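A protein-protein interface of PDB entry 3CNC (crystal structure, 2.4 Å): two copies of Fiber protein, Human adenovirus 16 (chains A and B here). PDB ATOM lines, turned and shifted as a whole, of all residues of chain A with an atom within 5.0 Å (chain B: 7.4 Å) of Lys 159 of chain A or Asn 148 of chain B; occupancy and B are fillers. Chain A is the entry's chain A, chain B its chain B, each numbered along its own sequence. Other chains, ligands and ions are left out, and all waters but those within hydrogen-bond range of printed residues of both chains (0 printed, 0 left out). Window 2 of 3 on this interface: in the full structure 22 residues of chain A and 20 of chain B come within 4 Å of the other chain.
Tyr 153 of chain B touches Tyr 157 of chain A.
Asn 148 of chain B touches Lys 159 of chain A (ND2 to O, 3.5 Å).
OH of Tyr 153 of chain B touches CD of Lys 159 of chain A, at 3.5 Å.
Leu 165 of chain A touches Tyr 153 of chain B.
Asn 148 of chain B touches Ile 207 of chain A (CB to CD1, 3.5 Å).
Printed residues of chain B within 4 Å of Tyr 157 of chain A: Tyr 153 (3.5 Å).
Lys 159 of chain A touches just these residues of chain B: Asn 148 (3.5 Å) and Tyr 153 (3.5 Å).
Ser 160 of chain A touches none of the printed residues of chain B.
Of the printed residues of chain A, Asn 148 of chain B touches Lys 159 (3.5 Å) and Ile 207 (3.5 Å).
Of the printed residues of chain A, Tyr 153 of chain B touches Tyr 157 (3.5 Å), Lys 159 (3.5 Å) and Leu 165 (3.6 Å).
Arg 176 of chain B touches none of the printed residues of chain A.
The nearest printed residue of chain A that does not touch Asn 148 of chain B is Ser 160 of chain A (5.0 Å).
Of the 10 printed residues of chain B, 2 touch a printed residue of chain A.
Hydrophobic or aromatic side chains of chain B within 4 Å of the printed part of chain A: Tyr 153.
Of the 10 printed residues of chain A, 4 touch a printed residue of chain B.
Hydrophobic or aromatic side chains of chain A that line the printed part of chain B: Tyr 157, Leu 165 and Ile 207.
Along chain A the printed residues that touch a printed residue of chain B span positions 157 to 207.
Among the printed residues, no Asp or Glu carboxylate lies within 4 Å of a Lys or Arg side-chain nitrogen of the other chain.
No position is printed for both chains.
Of the 5 pairs that touch across the chains among the printed residues, none has its exchanged pair printed and touching as well.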
ATOM      1  N   TYR A 157     -22.458  12.353  14.101  1.00  0.00           N
ATOM      2  CA  TYR A 157     -21.786  13.645  14.229  1.00  0.00           C
ATOM      3  C   TYR A 157     -21.200  14.295  12.993  1.00  0.00           C
ATOM      4  O   TYR A 157     -20.967  13.661  11.965  1.00  0.00           O
ATOM      5  CB  TYR A 157     -20.660  13.549  15.271  1.00  0.00           C
ATOM      6  CG  TYR A 157     -21.130  13.086  16.620  1.00  0.00           C
ATOM      7  CD1 TYR A 157     -21.402  11.739  16.860  1.00  0.00           C
ATOM      8  CD2 TYR A 157     -21.392  14.002  17.631  1.00  0.00           C
ATOM      9  CE1 TYR A 157     -21.935  11.318  18.077  1.00  0.00           C
ATOM     10  CE2 TYR A 157     -21.923  13.599  18.845  1.00  0.00           C
ATOM     11  CZ  TYR A 157     -22.196  12.256  19.063  1.00  0.00           C
ATOM     12  OH  TYR A 157     -22.738  11.862  20.268  1.00  0.00           O
ATOM     13  N   TYR A 158     -20.962  15.594  13.128  1.00  0.00           N
ATOM     14  CA  TYR A 158     -20.337  16.375  12.079  1.00  0.00           C
ATOM     15  C   TYR A 158     -19.099  16.992  12.722  1.00  0.00           C
ATOM     16  O   TYR A 158     -19.193  17.619  13.775  1.00  0.00           O
ATOM     17  CB  TYR A 158     -21.255  17.486  11.591  1.00  0.00           C
ATOM     18  CG  TYR A 158     -20.538  18.424  10.654  1.00  0.00           C
ATOM     19  CD1 TYR A 158     -20.201  18.021   9.360  1.00  0.00           C
ATOM     20  CD2 TYR A 158     -20.142  19.694  11.077  1.00  0.00           C
ATOM     21  CE1 TYR A 158     -19.490  18.858   8.513  1.00  0.00           C
ATOM     22  CE2 TYR A 158     -19.427  20.536  10.235  1.00  0.00           C
ATOM     23  CZ  TYR A 158     -19.108  20.111   8.960  1.00  0.00           C
ATOM     24  OH  TYR A 158     -18.410  20.940   8.130  1.00  0.00           O
ATOM     25  N   LYS A 159     -17.941  16.790  12.102  1.00  0.00           N
ATOM     26  CA  LYS A 159     -16.690  17.340  12.620  1.00  0.00           C
ATOM     27  C   LYS A 159     -16.367  18.607  11.829  1.00  0.00           C
ATOM     28  O   LYS A 159     -16.089  18.539  10.630  1.00  0.00           O
ATOM     29  CB  LYS A 159     -15.556  16.325  12.455  1.00  0.00           C
ATOM     30  CG  LYS A 159     -14.241  16.730  13.113  1.00  0.00           C
ATOM     31  CD  LYS A 159     -13.132  15.766  12.715  1.00  0.00           C
ATOM     32  CE  LYS A 159     -11.786  16.164  13.298  1.00  0.00           C
ATOM     33  NZ  LYS A 159     -10.677  15.425  12.627  1.00  0.00           N
ATOM     34  N   SER A 160     -16.400  19.756  12.496  1.00  0.00           N
ATOM     35  CA  SER A 160     -16.127  21.019  11.815  1.00  0.00           C
ATOM     36  C   SER A 160     -14.651  21.233  11.524  1.00  0.00           C
ATOM     37  O   SER A 160     -13.786  20.506  12.025  1.00  0.00           O
ATOM     38  CB  SER A 160     -16.656  22.207  12.624  1.00  0.00           C
ATOM     39  OG  SER A 160     -15.774  22.535  13.676  1.00  0.00           O
ATOM     40  N   THR A 161     -14.375  22.249  10.713  1.00  0.00           N
ATOM     41  CA  THR A 161     -13.014  22.583  10.316  1.00  0.00           C
ATOM     42  C   THR A 161     -12.052  22.761  11.493  1.00  0.00           C
ATOM     43  O   THR A 161     -10.907  22.328  11.420  1.00  0.00           O
ATOM     44  CB  THR A 161     -12.997  23.854   9.437  1.00  0.00           C
ATOM     45  OG1 THR A 161     -13.751  23.611   8.243  1.00  0.00           O
ATOM     46  CG2 THR A 161     -11.568  24.221   9.044  1.00  0.00           C
ATOM     47  N   GLY A 163     -12.268  21.296  14.262  1.00  0.00           N
ATOM     48  CA  GLY A 163     -12.212  20.069  15.039  1.00  0.00           C
ATOM     49  C   GLY A 163     -13.311  19.824  16.058  1.00  0.00           C
ATOM     50  O   GLY A 163     -13.255  18.838  16.790  1.00  0.00           O
ATOM     51  N   THR A 164     -14.308  20.699  16.121  1.00  0.00           N
ATOM     52  CA  THR A 164     -15.395  20.515  17.080  1.00  0.00           C
ATOM     53  C   THR A 164     -16.465  19.555  16.558  1.00  0.00           C
ATOM     54  O   THR A 164     -16.788  19.545  15.368  1.00  0.00           O
ATOM     55  CB  THR A 164     -16.062  21.861  17.454  1.00  0.00           C
ATOM     56  OG1 THR A 164     -16.384  22.583  16.259  1.00  0.00           O
ATOM     57  CG2 THR A 164     -15.131  22.701  18.324  1.00  0.00           C
ATOM     58  N   LEU A 165     -17.007  18.745  17.462  1.00  0.00           N
ATOM     59  CA  LEU A 165     -18.028  17.770  17.109  1.00  0.00           C
ATOM     60  C   LEU A 165     -19.439  18.275  17.369  1.00  0.00           C
ATOM     61  O   LEU A 165     -19.812  18.556  18.511  1.00  0.00           O
ATOM     62  CB  LEU A 165     -17.820  16.477  17.897  1.00  0.00           C
ATOM     63  CG  LEU A 165     -16.556  15.676  17.605  1.00  0.00           C
ATOM     64  CD1 LEU A 165     -16.488  14.491  18.571  1.00  0.00           C
ATOM     65  CD2 LEU A 165     -16.566  15.197  16.159  1.00  0.00           C
ATOM     66  N   GLU A 200     -19.704  25.901  10.440  1.00  0.00           N
ATOM     67  CA  GLU A 200     -18.737  26.445   9.493  1.00  0.00           C
ATOM     68  C   GLU A 200     -19.015  27.899   9.093  1.00  0.00           C
ATOM     69  O   GLU A 200     -20.000  28.508   9.521  1.00  0.00           O
ATOM     70  CB  GLU A 200     -18.687  25.595   8.217  1.00  0.00           C
ATOM     71  CG  GLU A 200     -18.300  24.126   8.399  1.00  0.00           C
ATOM     72  CD  GLU A 200     -16.968  23.922   9.108  1.00  0.00           C
ATOM     73  OE1 GLU A 200     -16.069  24.785   8.998  1.00  0.00           O
ATOM     74  OE2 GLU A 200     -16.819  22.876   9.768  1.00  0.00           O
ATOM     75  N   ILE A 207     -20.077  15.981   5.966  1.00  0.00           N
ATOM     76  CA  ILE A 207     -19.862  14.579   6.297  1.00  0.00           C
ATOM     77  C   ILE A 207     -20.591  14.204   7.587  1.00  0.00           C
ATOM     78  O   ILE A 207     -20.321  14.776   8.646  1.00  0.00           O
ATOM     79  CB  ILE A 207     -18.348  14.276   6.505  1.00  0.00           C
ATOM     80  CG1 ILE A 207     -17.565  14.609   5.231  1.00  0.00           C
ATOM     81  CG2 ILE A 207     -18.145  12.798   6.890  1.00  0.00           C
ATOM     82  CD1 ILE A 207     -16.051  14.460   5.385  1.00  0.00           C
ATOM     83  N   GLU B 145      -4.385  16.662   4.372  1.00  0.00           N
ATOM     84  CA  GLU B 145      -5.583  15.891   4.036  1.00  0.00           C
ATOM     85  C   GLU B 145      -6.324  15.472   5.300  1.00  0.00           C
ATOM     86  O   GLU B 145      -5.743  14.885   6.200  1.00  0.00           O
ATOM     87  CB  GLU B 145      -5.215  14.673   3.190  1.00  0.00           C
ATOM     88  CG  GLU B 145      -6.410  14.038   2.521  1.00  0.00           C
ATOM     89  CD  GLU B 145      -6.018  13.039   1.462  1.00  0.00           C
ATOM     90  OE1 GLU B 145      -5.033  12.309   1.677  1.00  0.00           O
ATOM     91  OE2 GLU B 145      -6.699  12.973   0.418  1.00  0.00           O
ATOM     92  N   THR B 146      -7.612  15.783   5.365  1.00  0.00           N
ATOM     93  CA  THR B 146      -8.411  15.469   6.543  1.00  0.00           C
ATOM     94  C   THR B 146      -9.021  14.062   6.621  1.00  0.00           C
ATOM     95  O   THR B 146      -8.835  13.356   7.614  1.00  0.00           O
ATOM     96  CB  THR B 146      -9.524  16.501   6.693  1.00  0.00           C
ATOM     97  OG1 THR B 146     -10.279  16.551   5.479  1.00  0.00           O
ATOM     98  CG2 THR B 146      -8.931  17.878   6.968  1.00  0.00           C
ATOM     99  N   LEU B 147      -9.748  13.665   5.582  1.00  0.00           N
ATOM    100  CA  LEU B 147     -10.397  12.349   5.527  1.00  0.00           C
ATOM    101  C   LEU B 147     -11.304  12.113   6.724  1.00  0.00           C
ATOM    102  O   LEU B 147     -11.127  11.135   7.464  1.00  0.00           O
ATOM    103  CB  LEU B 147      -9.354  11.226   5.458  1.00  0.00           C
ATOM    104  CG  LEU B 147      -8.532  11.101   4.174  1.00  0.00           C
ATOM    105  CD1 LEU B 147      -7.704   9.831   4.230  1.00  0.00           C
ATOM    106  CD2 LEU B 147      -9.451  11.071   2.968  1.00  0.00           C
ATOM    107  N   ASN B 148     -12.288  12.992   6.900  1.00  0.00           N
ATOM    108  CA  ASN B 148     -13.193  12.878   8.031  1.00  0.00           C
ATOM    109  C   ASN B 148     -14.144  11.680   7.994  1.00  0.00           C
ATOM    110  O   ASN B 148     -14.798  11.390   8.992  1.00  0.00           O
ATOM    111  CB  ASN B 148     -13.969  14.180   8.221  1.00  0.00           C
ATOM    112  CG  ASN B 148     -13.138  15.252   8.902  1.00  0.00           C
ATOM    113  OD1 ASN B 148     -11.996  15.011   9.306  1.00  0.00           O
ATOM    114  ND2 ASN B 148     -13.709  16.443   9.040  1.00  0.00           N
ATOM    115  N   GLU B 149     -14.211  10.983   6.860  1.00  0.00           N
ATOM    116  CA  GLU B 149     -15.061   9.794   6.755  1.00  0.00           C
ATOM    117  C   GLU B 149     -14.383   8.642   7.487  1.00  0.00           C
ATOM    118  O   GLU B 149     -14.960   7.566   7.602  1.00  0.00           O
ATOM    119  CB  GLU B 149     -15.242   9.332   5.311  1.00  0.00           C
ATOM    120  CG  GLU B 149     -15.112  10.403   4.295  1.00  0.00           C
ATOM    121  CD  GLU B 149     -13.686  10.600   3.814  1.00  0.00           C
ATOM    122  OE1 GLU B 149     -13.277   9.928   2.845  1.00  0.00           O
ATOM    123  OE2 GLU B 149     -12.988  11.435   4.414  1.00  0.00           O
ATOM    124  N   ASP B 150     -13.155   8.854   7.949  1.00  0.00           N
ATOM    125  CA  ASP B 150     -12.424   7.788   8.632  1.00  0.00           C
ATOM    126  C   ASP B 150     -12.740   7.662  10.118  1.00  0.00           C
ATOM    127  O   ASP B 150     -12.172   6.814  10.804  1.00  0.00           O
ATOM    128  CB  ASP B 150     -10.915   7.961   8.420  1.00  0.00           C
ATOM    129  CG  ASP B 150     -10.484   7.598   6.999  1.00  0.00           C
ATOM    130  OD1 ASP B 150     -11.367   7.238   6.177  1.00  0.00           O
ATOM    131  OD2 ASP B 150      -9.268   7.662   6.703  1.00  0.00           O
ATOM    132  N   TYR B 151     -13.669   8.486  10.597  1.00  0.00           N
ATOM    133  CA  TYR B 151     -14.042   8.464  12.001  1.00  0.00           C
ATOM    134  C   TYR B 151     -15.447   7.967  12.318  1.00  0.00           C
ATOM    135  O   TYR B 151     -16.390   8.118  11.535  1.00  0.00           O
ATOM    136  CB  TYR B 151     -13.881   9.853  12.619  1.00  0.00           C
ATOM    137  CG  TYR B 151     -12.497  10.421  12.492  1.00  0.00           C
ATOM    138  CD1 TYR B 151     -12.113  11.116  11.344  1.00  0.00           C
ATOM    139  CD2 TYR B 151     -11.554  10.245  13.504  1.00  0.00           C
ATOM    140  CE1 TYR B 151     -10.822  11.621  11.207  1.00  0.00           C
ATOM    141  CE2 TYR B 151     -10.259  10.745  13.377  1.00  0.00           C
ATOM    142  CZ  TYR B 151      -9.899  11.431  12.223  1.00  0.00           C
ATOM    143  OH  TYR B 151      -8.616  11.915  12.074  1.00  0.00           O
ATOM    144  N   ILE B 152     -15.567   7.379  13.499  1.00  0.00           N
ATOM    145  CA  ILE B 152     -16.828   6.881  14.009  1.00  0.00           C
ATOM    146  C   ILE B 152     -16.877   7.482  15.406  1.00  0.00           C
ATOM    147  O   ILE B 152     -15.883   7.427  16.128  1.00  0.00           O
ATOM    148  CB  ILE B 152     -16.817   5.337  14.098  1.00  0.00           C
ATOM    149  CG1 ILE B 152     -16.995   4.732  12.708  1.00  0.00           C
ATOM    150  CG2 ILE B 152     -17.904   4.844  15.052  1.00  0.00           C
ATOM    151  CD1 ILE B 152     -16.842   3.215  12.683  1.00  0.00           C
ATOM    152  N   TYR B 153     -17.994   8.104  15.768  1.00  0.00           N
ATOM    153  CA  TYR B 153     -18.128   8.674  17.100  1.00  0.00           C
ATOM    154  C   TYR B 153     -19.318   8.017  17.791  1.00  0.00           C
ATOM    155  O   TYR B 153     -20.290   7.606  17.145  1.00  0.00           O
ATOM    156  CB  TYR B 153     -18.324  10.191  17.042  1.00  0.00           C
ATOM    157  CG  TYR B 153     -17.327  10.899  16.152  1.00  0.00           C
ATOM    158  CD1 TYR B 153     -17.607  11.113  14.805  1.00  0.00           C
ATOM    159  CD2 TYR B 153     -16.089  11.324  16.644  1.00  0.00           C
ATOM    160  CE1 TYR B 153     -16.691  11.730  13.965  1.00  0.00           C
ATOM    161  CE2 TYR B 153     -15.154  11.951  15.804  1.00  0.00           C
ATOM    162  CZ  TYR B 153     -15.469  12.148  14.462  1.00  0.00           C
ATOM    163  OH  TYR B 153     -14.583  12.761  13.603  1.00  0.00           O
ATOM    164  N   ARG B 176      -6.527   5.548   7.578  1.00  0.00           N
ATOM    165  CA  ARG B 176      -6.155   6.960   7.555  1.00  0.00           C
ATOM    166  C   ARG B 176      -4.656   7.295   7.607  1.00  0.00           C
ATOM    167  O   ARG B 176      -4.105   7.848   6.659  1.00  0.00           O
ATOM    168  CB  ARG B 176      -6.865   7.713   8.690  1.00  0.00           C
ATOM    169  CG  ARG B 176      -6.924   9.209   8.452  1.00  0.00           C
ATOM    170  CD  ARG B 176      -7.629   9.990   9.548  1.00  0.00           C
ATOM    171  NE  ARG B 176      -6.659  10.579  10.462  1.00  0.00           N
ATOM    172  CZ  ARG B 176      -5.840  11.574  10.135  1.00  0.00           C
ATOM    173  NH1 ARG B 176      -5.886  12.101   8.917  1.00  0.00           N
ATOM    174  NH2 ARG B 176      -4.954  12.022  11.013  1.00  0.00           N
